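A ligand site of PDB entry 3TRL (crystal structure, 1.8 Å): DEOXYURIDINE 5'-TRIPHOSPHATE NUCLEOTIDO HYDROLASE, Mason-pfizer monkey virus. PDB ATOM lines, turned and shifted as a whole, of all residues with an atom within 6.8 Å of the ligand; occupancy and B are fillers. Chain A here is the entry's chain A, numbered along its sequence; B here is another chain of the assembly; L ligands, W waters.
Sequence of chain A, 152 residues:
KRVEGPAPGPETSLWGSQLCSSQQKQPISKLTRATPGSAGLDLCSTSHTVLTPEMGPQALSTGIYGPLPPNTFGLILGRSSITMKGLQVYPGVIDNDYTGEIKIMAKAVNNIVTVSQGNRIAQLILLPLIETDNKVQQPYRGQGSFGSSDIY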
ATOM      1  N   ILE A  76      -1.114  21.644   7.320  1.00  0.00           N
ATOM      2  CA  ILE A  76      -2.273  21.933   8.157  1.00  0.00           C
ATOM      3  C   ILE A  76      -2.738  23.343   7.828  1.00  0.00           C
ATOM      4  O   ILE A  76      -1.959  24.270   7.942  1.00  0.00           O
ATOM      5  CB  ILE A  76      -1.876  21.922   9.652  1.00  0.00           C
ATOM      6  CG1 ILE A  76      -1.134  20.625   9.975  1.00  0.00           C
ATOM      7  CG2 ILE A  76      -3.123  22.041  10.551  1.00  0.00           C
ATOM      8  CD1 ILE A  76      -1.881  19.449   9.559  1.00  0.00           C
ATOM      9  N   VAL A  89      -5.611  29.526  12.216  1.00  0.00           N
ATOM     10  CA  VAL A  89      -4.708  28.364  12.286  1.00  0.00           C
ATOM     11  C   VAL A  89      -3.476  28.774  11.505  1.00  0.00           C
ATOM     12  O   VAL A  89      -3.556  29.216  10.338  1.00  0.00           O
ATOM     13  CB  VAL A  89      -5.413  27.079  11.702  1.00  0.00           C
ATOM     14  CG1 VAL A  89      -4.406  25.973  11.318  1.00  0.00           C
ATOM     15  CG2 VAL A  89      -6.425  26.533  12.706  1.00  0.00           C
ATOM     16  N   TYR A  90      -2.307  28.632  12.095  1.00  0.00           N
ATOM     17  CA  TYR A  90      -1.079  28.970  11.383  1.00  0.00           C
ATOM     18  C   TYR A  90      -0.741  27.772  10.490  1.00  0.00           C
ATOM     19  O   TYR A  90      -0.711  26.641  10.962  1.00  0.00           O
ATOM     20  CB  TYR A  90       0.058  29.154  12.370  1.00  0.00           C
ATOM     21  CG  TYR A  90      -0.144  30.347  13.297  1.00  0.00           C
ATOM     22  CD1 TYR A  90      -0.030  31.645  12.807  1.00  0.00           C
ATOM     23  CD2 TYR A  90      -0.477  30.171  14.666  1.00  0.00           C
ATOM     24  CE1 TYR A  90      -0.211  32.798  13.679  1.00  0.00           C
ATOM     25  CE2 TYR A  90      -0.676  31.288  15.542  1.00  0.00           C
ATOM     26  CZ  TYR A  90      -0.529  32.588  15.029  1.00  0.00           C
ATOM     27  OH  TYR A  90      -0.696  33.708  15.824  1.00  0.00           O
ATOM     28  N   PRO A  91      -0.485  28.019   9.204  1.00  0.00           N
ATOM     29  CA  PRO A  91      -0.158  26.906   8.283  1.00  0.00           C
ATOM     30  C   PRO A  91       1.053  26.115   8.822  1.00  0.00           C
ATOM     31  O   PRO A  91       2.059  26.721   9.198  1.00  0.00           O
ATOM     32  CB  PRO A  91       0.207  27.629   6.980  1.00  0.00           C
ATOM     33  CG  PRO A  91      -0.640  28.893   7.035  1.00  0.00           C
ATOM     34  CD  PRO A  91      -0.564  29.313   8.507  1.00  0.00           C
ATOM     35  N   GLY A  92       0.957  24.795   8.870  1.00  0.00           N
ATOM     36  CA  GLY A  92       2.038  24.022   9.462  1.00  0.00           C
ATOM     37  C   GLY A  92       2.413  22.892   8.497  1.00  0.00           C
ATOM     38  O   GLY A  92       1.518  22.231   7.943  1.00  0.00           O
ATOM     39  N   VAL A  93       3.726  22.676   8.357  1.00  0.00           N
ATOM     40  CA  VAL A  93       4.293  21.657   7.480  1.00  0.00           C
ATOM     41  C   VAL A  93       4.421  20.338   8.269  1.00  0.00           C
ATOM     42  O   VAL A  93       5.022  20.326   9.344  1.00  0.00           O
ATOM     43  CB  VAL A  93       5.698  22.118   7.083  1.00  0.00           C
ATOM     44  CG1 VAL A  93       6.429  21.054   6.286  1.00  0.00           C
ATOM     45  CG2 VAL A  93       5.603  23.454   6.270  1.00  0.00           C
ATOM     46  N   ILE A  94       3.888  19.243   7.737  1.00  0.00           N
ATOM     47  CA  ILE A  94       4.092  17.966   8.402  1.00  0.00           C
ATOM     48  C   ILE A  94       5.076  17.190   7.535  1.00  0.00           C
ATOM     49  O   ILE A  94       4.807  16.852   6.366  1.00  0.00           O
ATOM     50  CB  ILE A  94       2.744  17.165   8.507  1.00  0.00           C
ATOM     51  CG1 ILE A  94       1.592  18.003   9.107  1.00  0.00           C
ATOM     52  CG2 ILE A  94       2.897  15.847   9.328  1.00  0.00           C
ATOM     53  CD1 ILE A  94       1.900  18.761  10.428  1.00  0.00           C
ATOM     54  N   ASP A  95       6.190  16.824   8.120  1.00  0.00           N
ATOM     55  CA  ASP A  95       7.206  16.141   7.339  1.00  0.00           C
ATOM     56  C   ASP A  95       6.790  14.732   7.052  1.00  0.00           C
ATOM     57  O   ASP A  95       6.069  14.096   7.839  1.00  0.00           O
ATOM     58  CB  ASP A  95       8.547  16.179   8.045  1.00  0.00           C
ATOM     59  CG  ASP A  95       9.056  17.646   8.225  1.00  0.00           C
ATOM     60  OD1 ASP A  95       9.176  18.369   7.208  1.00  0.00           O
ATOM     61  OD2 ASP A  95       9.248  18.085   9.378  1.00  0.00           O
ATOM     62  N   ASN A  96       7.276  14.214   5.939  1.00  0.00           N
ATOM     63  CA  ASN A  96       6.916  12.831   5.540  1.00  0.00           C
ATOM     64  C   ASN A  96       7.152  11.778   6.630  1.00  0.00           C
ATOM     65  O   ASN A  96       6.319  10.851   6.815  1.00  0.00           O
ATOM     66  CB  ASN A  96       7.664  12.390   4.267  1.00  0.00           C
ATOM     67  CG  ASN A  96       7.297  10.965   3.866  1.00  0.00           C
ATOM     68  OD1 ASN A  96       8.041  10.016   4.146  1.00  0.00           O
ATOM     69  ND2 ASN A  96       6.110  10.816   3.259  1.00  0.00           N
ATOM     70  N   ASP A  97       8.264  11.914   7.333  1.00  0.00           N
ATOM     71  CA  ASP A  97       8.687  10.883   8.315  1.00  0.00           C
ATOM     72  C   ASP A  97       8.436  11.287   9.746  1.00  0.00           C
ATOM     73  O   ASP A  97       8.969  10.668  10.675  1.00  0.00           O
ATOM     74  CB  ASP A  97      10.162  10.587   8.147  1.00  0.00           C
ATOM     75  CG  ASP A  97      11.048  11.870   8.192  1.00  0.00           C
ATOM     76  OD1 ASP A  97      10.566  13.039   8.362  1.00  0.00           O
ATOM     77  OD2 ASP A  97      12.251  11.683   8.029  1.00  0.00           O
ATOM     78  N   TYR A  98       7.613  12.309   9.956  1.00  0.00           N
ATOM     79  CA  TYR A  98       7.222  12.647  11.336  1.00  0.00           C
ATOM     80  C   TYR A  98       6.344  11.540  11.967  1.00  0.00           C
ATOM     81  O   TYR A  98       5.359  11.136  11.355  1.00  0.00           O
ATOM     82  CB  TYR A  98       6.365  13.905  11.253  1.00  0.00           C
ATOM     83  CG  TYR A  98       5.869  14.405  12.578  1.00  0.00           C
ATOM     84  CD1 TYR A  98       6.746  14.918  13.527  1.00  0.00           C
ATOM     85  CD2 TYR A  98       4.487  14.415  12.875  1.00  0.00           C
ATOM     86  CE1 TYR A  98       6.285  15.429  14.750  1.00  0.00           C
ATOM     87  CE2 TYR A  98       4.016  14.933  14.091  1.00  0.00           C
ATOM     88  CZ  TYR A  98       4.927  15.434  15.015  1.00  0.00           C
ATOM     89  OH  TYR A  98       4.431  15.951  16.198  1.00  0.00           O
ATOM     90  N   GLY A 100       5.237  11.731  15.298  1.00  0.00           N
ATOM     91  CA  GLY A 100       4.643  12.304  16.503  1.00  0.00           C
ATOM     92  C   GLY A 100       3.185  12.656  16.254  1.00  0.00           C
ATOM     93  O   GLY A 100       2.634  12.360  15.193  1.00  0.00           O
ATOM     94  N   GLU A 101       2.567  13.301  17.243  1.00  0.00           N
ATOM     95  CA  GLU A 101       1.200  13.749  17.159  1.00  0.00           C
ATOM     96  C   GLU A 101       1.130  15.037  16.342  1.00  0.00           C
ATOM     97  O   GLU A 101       1.907  15.999  16.521  1.00  0.00           O
ATOM     98  CB  GLU A 101       0.620  13.973  18.566  1.00  0.00           C
ATOM     99  CG  GLU A 101      -0.867  14.277  18.540  1.00  0.00           C
ATOM    100  CD  GLU A 101      -1.405  14.761  19.887  1.00  0.00           C
ATOM    101  OE1 GLU A 101      -0.621  14.812  20.855  1.00  0.00           O
ATOM    102  OE2 GLU A 101      -2.613  15.077  19.953  1.00  0.00           O
ATOM    103  N   ILE A 102       0.218  15.033  15.385  1.00  0.00           N
ATOM    104  CA  ILE A 102      -0.071  16.220  14.591  1.00  0.00           C
ATOM    105  C   ILE A 102      -0.840  17.196  15.480  1.00  0.00           C
ATOM    106  O   ILE A 102      -1.891  16.865  16.025  1.00  0.00           O
ATOM    107  CB  ILE A 102      -0.882  15.815  13.354  1.00  0.00           C
ATOM    108  CG1 ILE A 102       0.012  14.955  12.451  1.00  0.00           C
ATOM    109  CG2 ILE A 102      -1.385  17.057  12.601  1.00  0.00           C
ATOM    110  CD1 ILE A 102      -0.713  14.407  11.245  1.00  0.00           C
ATOM    111  N   LYS A 103      -0.279  18.361  15.725  1.00  0.00           N
ATOM    112  CA  LYS A 103      -0.985  19.363  16.516  1.00  0.00           C
ATOM    113  C   LYS A 103      -1.356  20.560  15.653  1.00  0.00           C
ATOM    114  O   LYS A 103      -0.718  20.845  14.638  1.00  0.00           O
ATOM    115  CB  LYS A 103      -0.097  19.846  17.680  1.00  0.00           C
ATOM    116  CG  LYS A 103       0.188  18.663  18.639  1.00  0.00           C
ATOM    117  CD  LYS A 103       0.382  19.142  20.037  1.00  0.00           C
ATOM    118  CE  LYS A 103       0.967  18.032  20.919  1.00  0.00           C
ATOM    119  NZ  LYS A 103       1.379  18.612  22.237  1.00  0.00           N
ATOM    120  N   ILE A 104      -2.384  21.267  16.097  1.00  0.00           N
ATOM    121  CA  ILE A 104      -2.874  22.397  15.314  1.00  0.00           C
ATOM    122  C   ILE A 104      -2.361  23.644  16.047  1.00  0.00           C
ATOM    123  O   ILE A 104      -2.553  23.778  17.273  1.00  0.00           O
ATOM    124  CB  ILE A 104      -4.416  22.407  15.252  1.00  0.00           C
ATOM    125  CG1 ILE A 104      -4.952  21.136  14.550  1.00  0.00           C
ATOM    126  CG2 ILE A 104      -4.928  23.683  14.548  1.00  0.00           C
ATOM    127  CD1 ILE A 104      -6.391  20.944  14.777  1.00  0.00           C
ATOM    128  N   MET A 105      -1.657  24.512  15.328  1.00  0.00           N
ATOM    129  CA  MET A 105      -1.153  25.768  15.910  1.00  0.00           C
ATOM    130  C   MET A 105      -2.193  26.859  15.639  1.00  0.00           C
ATOM    131  O   MET A 105      -2.478  27.172  14.481  1.00  0.00           O
ATOM    132  CB  MET A 105       0.165  26.162  15.248  1.00  0.00           C
ATOM    133  CG  MET A 105       1.261  25.091  15.399  1.00  0.00           C
ATOM    134  SD  MET A 105       2.857  25.745  14.855  1.00  0.00           S
ATOM    135  CE  MET A 105       2.546  25.943  13.041  1.00  0.00           C
ATOM    136  N   ALA B  39      10.140  18.181   4.565  1.00  0.00           N
ATOM    137  CA  ALA B  39       9.560  18.784   3.414  1.00  0.00           C
ATOM    138  C   ALA B  39      10.301  20.070   3.002  1.00  0.00           C
ATOM    139  O   ALA B  39      10.329  20.426   1.828  1.00  0.00           O
ATOM    140  CB  ALA B  39       8.106  19.087   3.707  1.00  0.00           C
ATOM    141  N   GLY B  40      10.855  20.807   3.973  1.00  0.00           N
ATOM    142  CA  GLY B  40      11.263  22.179   3.714  1.00  0.00           C
ATOM    143  C   GLY B  40      12.781  22.367   3.706  1.00  0.00           C
ATOM    144  O   GLY B  40      13.514  21.590   4.325  1.00  0.00           O
ATOM    145  N   ASP B  42      15.694  24.895   4.929  1.00  0.00           N
ATOM    146  CA  ASP B  42      15.759  25.936   5.978  1.00  0.00           C
ATOM    147  C   ASP B  42      16.253  27.276   5.431  1.00  0.00           C
ATOM    148  O   ASP B  42      17.215  27.298   4.672  1.00  0.00           O
ATOM    149  CB  ASP B  42      16.653  25.497   7.122  1.00  0.00           C
ATOM    150  CG  ASP B  42      16.247  24.170   7.689  1.00  0.00           C
ATOM    151  OD1 ASP B  42      15.091  24.060   8.153  1.00  0.00           O
ATOM    152  OD2 ASP B  42      17.083  23.239   7.619  1.00  0.00           O
ATOM    153  N   GLY B  78       6.346  29.103   7.939  1.00  0.00           N
ATOM    154  CA  GLY B  78       6.990  29.112   9.257  1.00  0.00           C
ATOM    155  C   GLY B  78       7.540  27.764   9.672  1.00  0.00           C
ATOM    156  O   GLY B  78       7.181  26.731   9.102  1.00  0.00           O
ATOM    157  N   ARG B  79       8.485  27.764  10.611  1.00  0.00           N
ATOM    158  CA  ARG B  79       8.874  26.535  11.298  1.00  0.00           C
ATOM    159  C   ARG B  79       7.996  26.514  12.512  1.00  0.00           C
ATOM    160  O   ARG B  79       7.809  27.556  13.138  1.00  0.00           O
ATOM    161  CB  ARG B  79      10.368  26.588  11.726  1.00  0.00           C
ATOM    162  CG  ARG B  79      11.307  26.344  10.572  1.00  0.00           C
ATOM    163  CD  ARG B  79      12.751  26.514  11.003  1.00  0.00           C
ATOM    164  NE  ARG B  79      13.124  25.368  11.832  1.00  0.00           N
ATOM    165  CZ  ARG B  79      13.721  25.432  13.030  1.00  0.00           C
ATOM    166  NH1 ARG B  79      14.079  26.614  13.539  1.00  0.00           N
ATOM    167  NH2 ARG B  79      13.996  24.302  13.695  1.00  0.00           N
ATOM    168  N   SER B  80       7.426  25.369  12.867  1.00  0.00           N
ATOM    169  CA  SER B  80       6.497  25.352  14.009  1.00  0.00           C
ATOM    170  C   SER B  80       7.134  25.800  15.307  1.00  0.00           C
ATOM    171  O   SER B  80       6.469  26.451  16.125  1.00  0.00           O
ATOM    172  CB  SER B  80       5.835  23.976  14.202  1.00  0.00           C
ATOM    173  OG  SER B  80       6.816  22.987  14.416  1.00  0.00           O
ATOM    174  N   SER B  81       8.403  25.464  15.515  1.00  0.00           N
ATOM    175  CA  SER B  81       9.035  25.833  16.818  1.00  0.00           C
ATOM    176  C   SER B  81       9.139  27.364  16.961  1.00  0.00           C
ATOM    177  O   SER B  81       9.035  27.895  18.088  1.00  0.00           O
ATOM    178  CB  SER B  81      10.395  25.143  16.995  1.00  0.00           C
ATOM    179  OG  SER B  81      11.255  25.692  15.997  1.00  0.00           O
ATOM    180  N   THR B  83       7.034  29.631  15.116  1.00  0.00           N
ATOM    181  CA  THR B  83       5.618  30.044  15.311  1.00  0.00           C
ATOM    182  C   THR B  83       5.182  29.951  16.788  1.00  0.00           C
ATOM    183  O   THR B  83       4.601  30.923  17.369  1.00  0.00           O
ATOM    184  CB  THR B  83       4.665  29.220  14.408  1.00  0.00           C
ATOM    185  OG1 THR B  83       5.155  29.272  13.066  1.00  0.00           O
ATOM    186  CG2 THR B  83       3.202  29.737  14.533  1.00  0.00           C
ATOM    187  N   GLN B 123      11.023  28.164   6.240  1.00  0.00           N
ATOM    188  CA  GLN B 123      11.390  27.046   5.389  1.00  0.00           C
ATOM    189  C   GLN B 123      10.830  27.263   4.010  1.00  0.00           C
ATOM    190  O   GLN B 123       9.759  27.804   3.872  1.00  0.00           O
ATOM    191  CB  GLN B 123      10.937  25.673   5.948  1.00  0.00           C
ATOM    192  CG  GLN B 123       9.416  25.524   6.229  1.00  0.00           C
ATOM    193  CD  GLN B 123       9.175  24.243   6.957  1.00  0.00           C
ATOM    194  OE1 GLN B 123       9.639  23.154   6.536  1.00  0.00           O
ATOM    195  NE2 GLN B 123       8.483  24.356   8.080  1.00  0.00           N
HETATM  196  N1  LIG L   1       3.949  19.909  13.273  1.00  0.00           N
HETATM  197  C1  LIG L   1       2.651  19.809  13.737  1.00  0.00           C
HETATM  198  N2  LIG L   1       1.737  20.817  13.476  1.00  0.00           N
HETATM  199  C2  LIG L   1       2.099  21.909  12.704  1.00  0.00           C
HETATM  200  C3  LIG L   1       3.415  21.996  12.199  1.00  0.00           C
HETATM  201  C4  LIG L   1       4.368  21.026  12.517  1.00  0.00           C
HETATM  202  O1  LIG L   1       2.275  18.837  14.475  1.00  0.00           O
HETATM  203  O2  LIG L   1       1.210  22.762  12.485  1.00  0.00           O
HETATM  204  C5  LIG L   1       4.943  18.857  13.567  1.00  0.00           C
HETATM  205  C6  LIG L   1       5.122  18.006  12.287  1.00  0.00           C
HETATM  206  C7  LIG L   1       6.394  18.553  11.650  1.00  0.00           C
HETATM  207  C8  LIG L   1       7.188  18.871  12.911  1.00  0.00           C
HETATM  208  O3  LIG L   1       6.995  17.521  10.893  1.00  0.00           O
HETATM  209  O4  LIG L   1       6.254  19.352  13.850  1.00  0.00           O
HETATM  210  C9  LIG L   1       8.295  19.889  12.754  1.00  0.00           C
HETATM  211  O5  LIG L   1       7.650  21.116  12.351  1.00  0.00           O
HETATM  212  P1  LIG L   1       8.345  22.018  11.202  1.00  0.00           P
HETATM  213  O6  LIG L   1       9.718  22.135  11.457  1.00  0.00           O
HETATM  214  O7  LIG L   1       8.086  21.164   9.943  1.00  0.00           O
HETATM  215  O8  LIG L   1       7.538  23.273  11.062  1.00  0.00           O
HETATM  216  O   HOH W   1      12.110  20.636  12.504  1.00  0.00           O
HETATM  217  O   HOH W   2       5.292  24.326  10.198  1.00  0.00           O
HETATM  218  O   HOH W   3      -1.122  24.330  12.571  1.00  0.00           O
HETATM  219  O   HOH W   4      10.403  23.318  13.787  1.00  0.00           O
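N of Lys 103 sits at hydrogen-bond distance from O1 of the ligand (2.9 Å).
An oxygen (O8) of the ligand lies within hydrogen-bond range of the backbone NH (N) of Ser 80 of chain B (2.8 Å).
An oxygen (O3) of the ligand is in hydrogen-bond range of the backbone NH (N) of Asp 95, 3.0 Å away.
An oxygen (O5) of the ligand lies within hydrogen-bond range of the side-chain hydroxyl (OG) of Ser 80 of chain B (2.9 Å).
O of Lys 103 lies within hydrogen-bond range of N2 of the ligand (2.7 Å).
The side-chain carboxylate (OD2) of Asp 95 sits at hydrogen-bond distance from an oxygen (O3) of the ligand.
An oxygen (O8) of the ligand is in hydrogen-bond range of the side-chain amide nitrogen (NE2) of Gln 123 of chain B, 3.3 Å away.
The backbone carbonyl oxygen (O) of Gly 92 is in hydrogen-bond range of the backbone NH (N) of Ile 76 (2.8 Å).
The backbone carbonyl oxygen (O) of Glu 101 is in hydrogen-bond range of the side-chain hydroxyl (OH) of Tyr 98.
O of Gly 78 of chain B lies within hydrogen-bond range of NE2 of Gln 123 of chain B, at 2.9 Å.
The backbone carbonyl oxygen (O) of Met 105 is in hydrogen-bond range of the backbone NH (N) of Tyr 90 (2.8 Å).
O of Arg 79 of chain B sits at hydrogen-bond distance from OG1 of Thr 83 of chain B (3.2 Å).
The side-chain carboxylate (OD1) of Asp 95 lies within hydrogen-bond range of the backbone NH (N) of Ala 39 of chain B, at 2.8 Å.
O of Val 93 sits close to O7 of the ligand, at 3.2 Å.
Gly 92 touches the ligand.
Ile 94 touches the ligand (CD1 to C1, 3.6 Å).
Tyr 98 touches the ligand.
Glu 101 touches the ligand.
Ile 102 touches the ligand (CA to O1, 3.5 Å).
CE of Met 105 touches O2 of the ligand (3.5 Å).
O of Gly 78 of chain B touches O8 of the ligand, 3.99 Å away.
Arg 79 of chain B touches the ligand.
13 residues have an atom within 4 Å of the ligand: Gly 92, Val 93, Ile 94, Asp 95, Tyr 98, Glu 101, Ile 102, Lys 103, Met 105, Gly 78 of chain B, Arg 79 of chain B, Ser 80 of chain B and Gln 123 of chain B.
The nearest printed residue that does not touch the ligand is Ile 76 (4.04 Å).
Water W2 lies within hydrogen-bond range of an oxygen (O8) of the ligand (2.6 Å), the backbone NH (N) of Val 93 (2.9 Å) and the backbone carbonyl oxygen (O) of Gly 78 of chain B (3.2 Å).
Water W4 lies within hydrogen-bond range of O6 of the ligand and OG of Ser 81 of chain B.
Water W3 lies within hydrogen-bond range of O2 of the ligand, N of Met 105 and O of Tyr 90.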
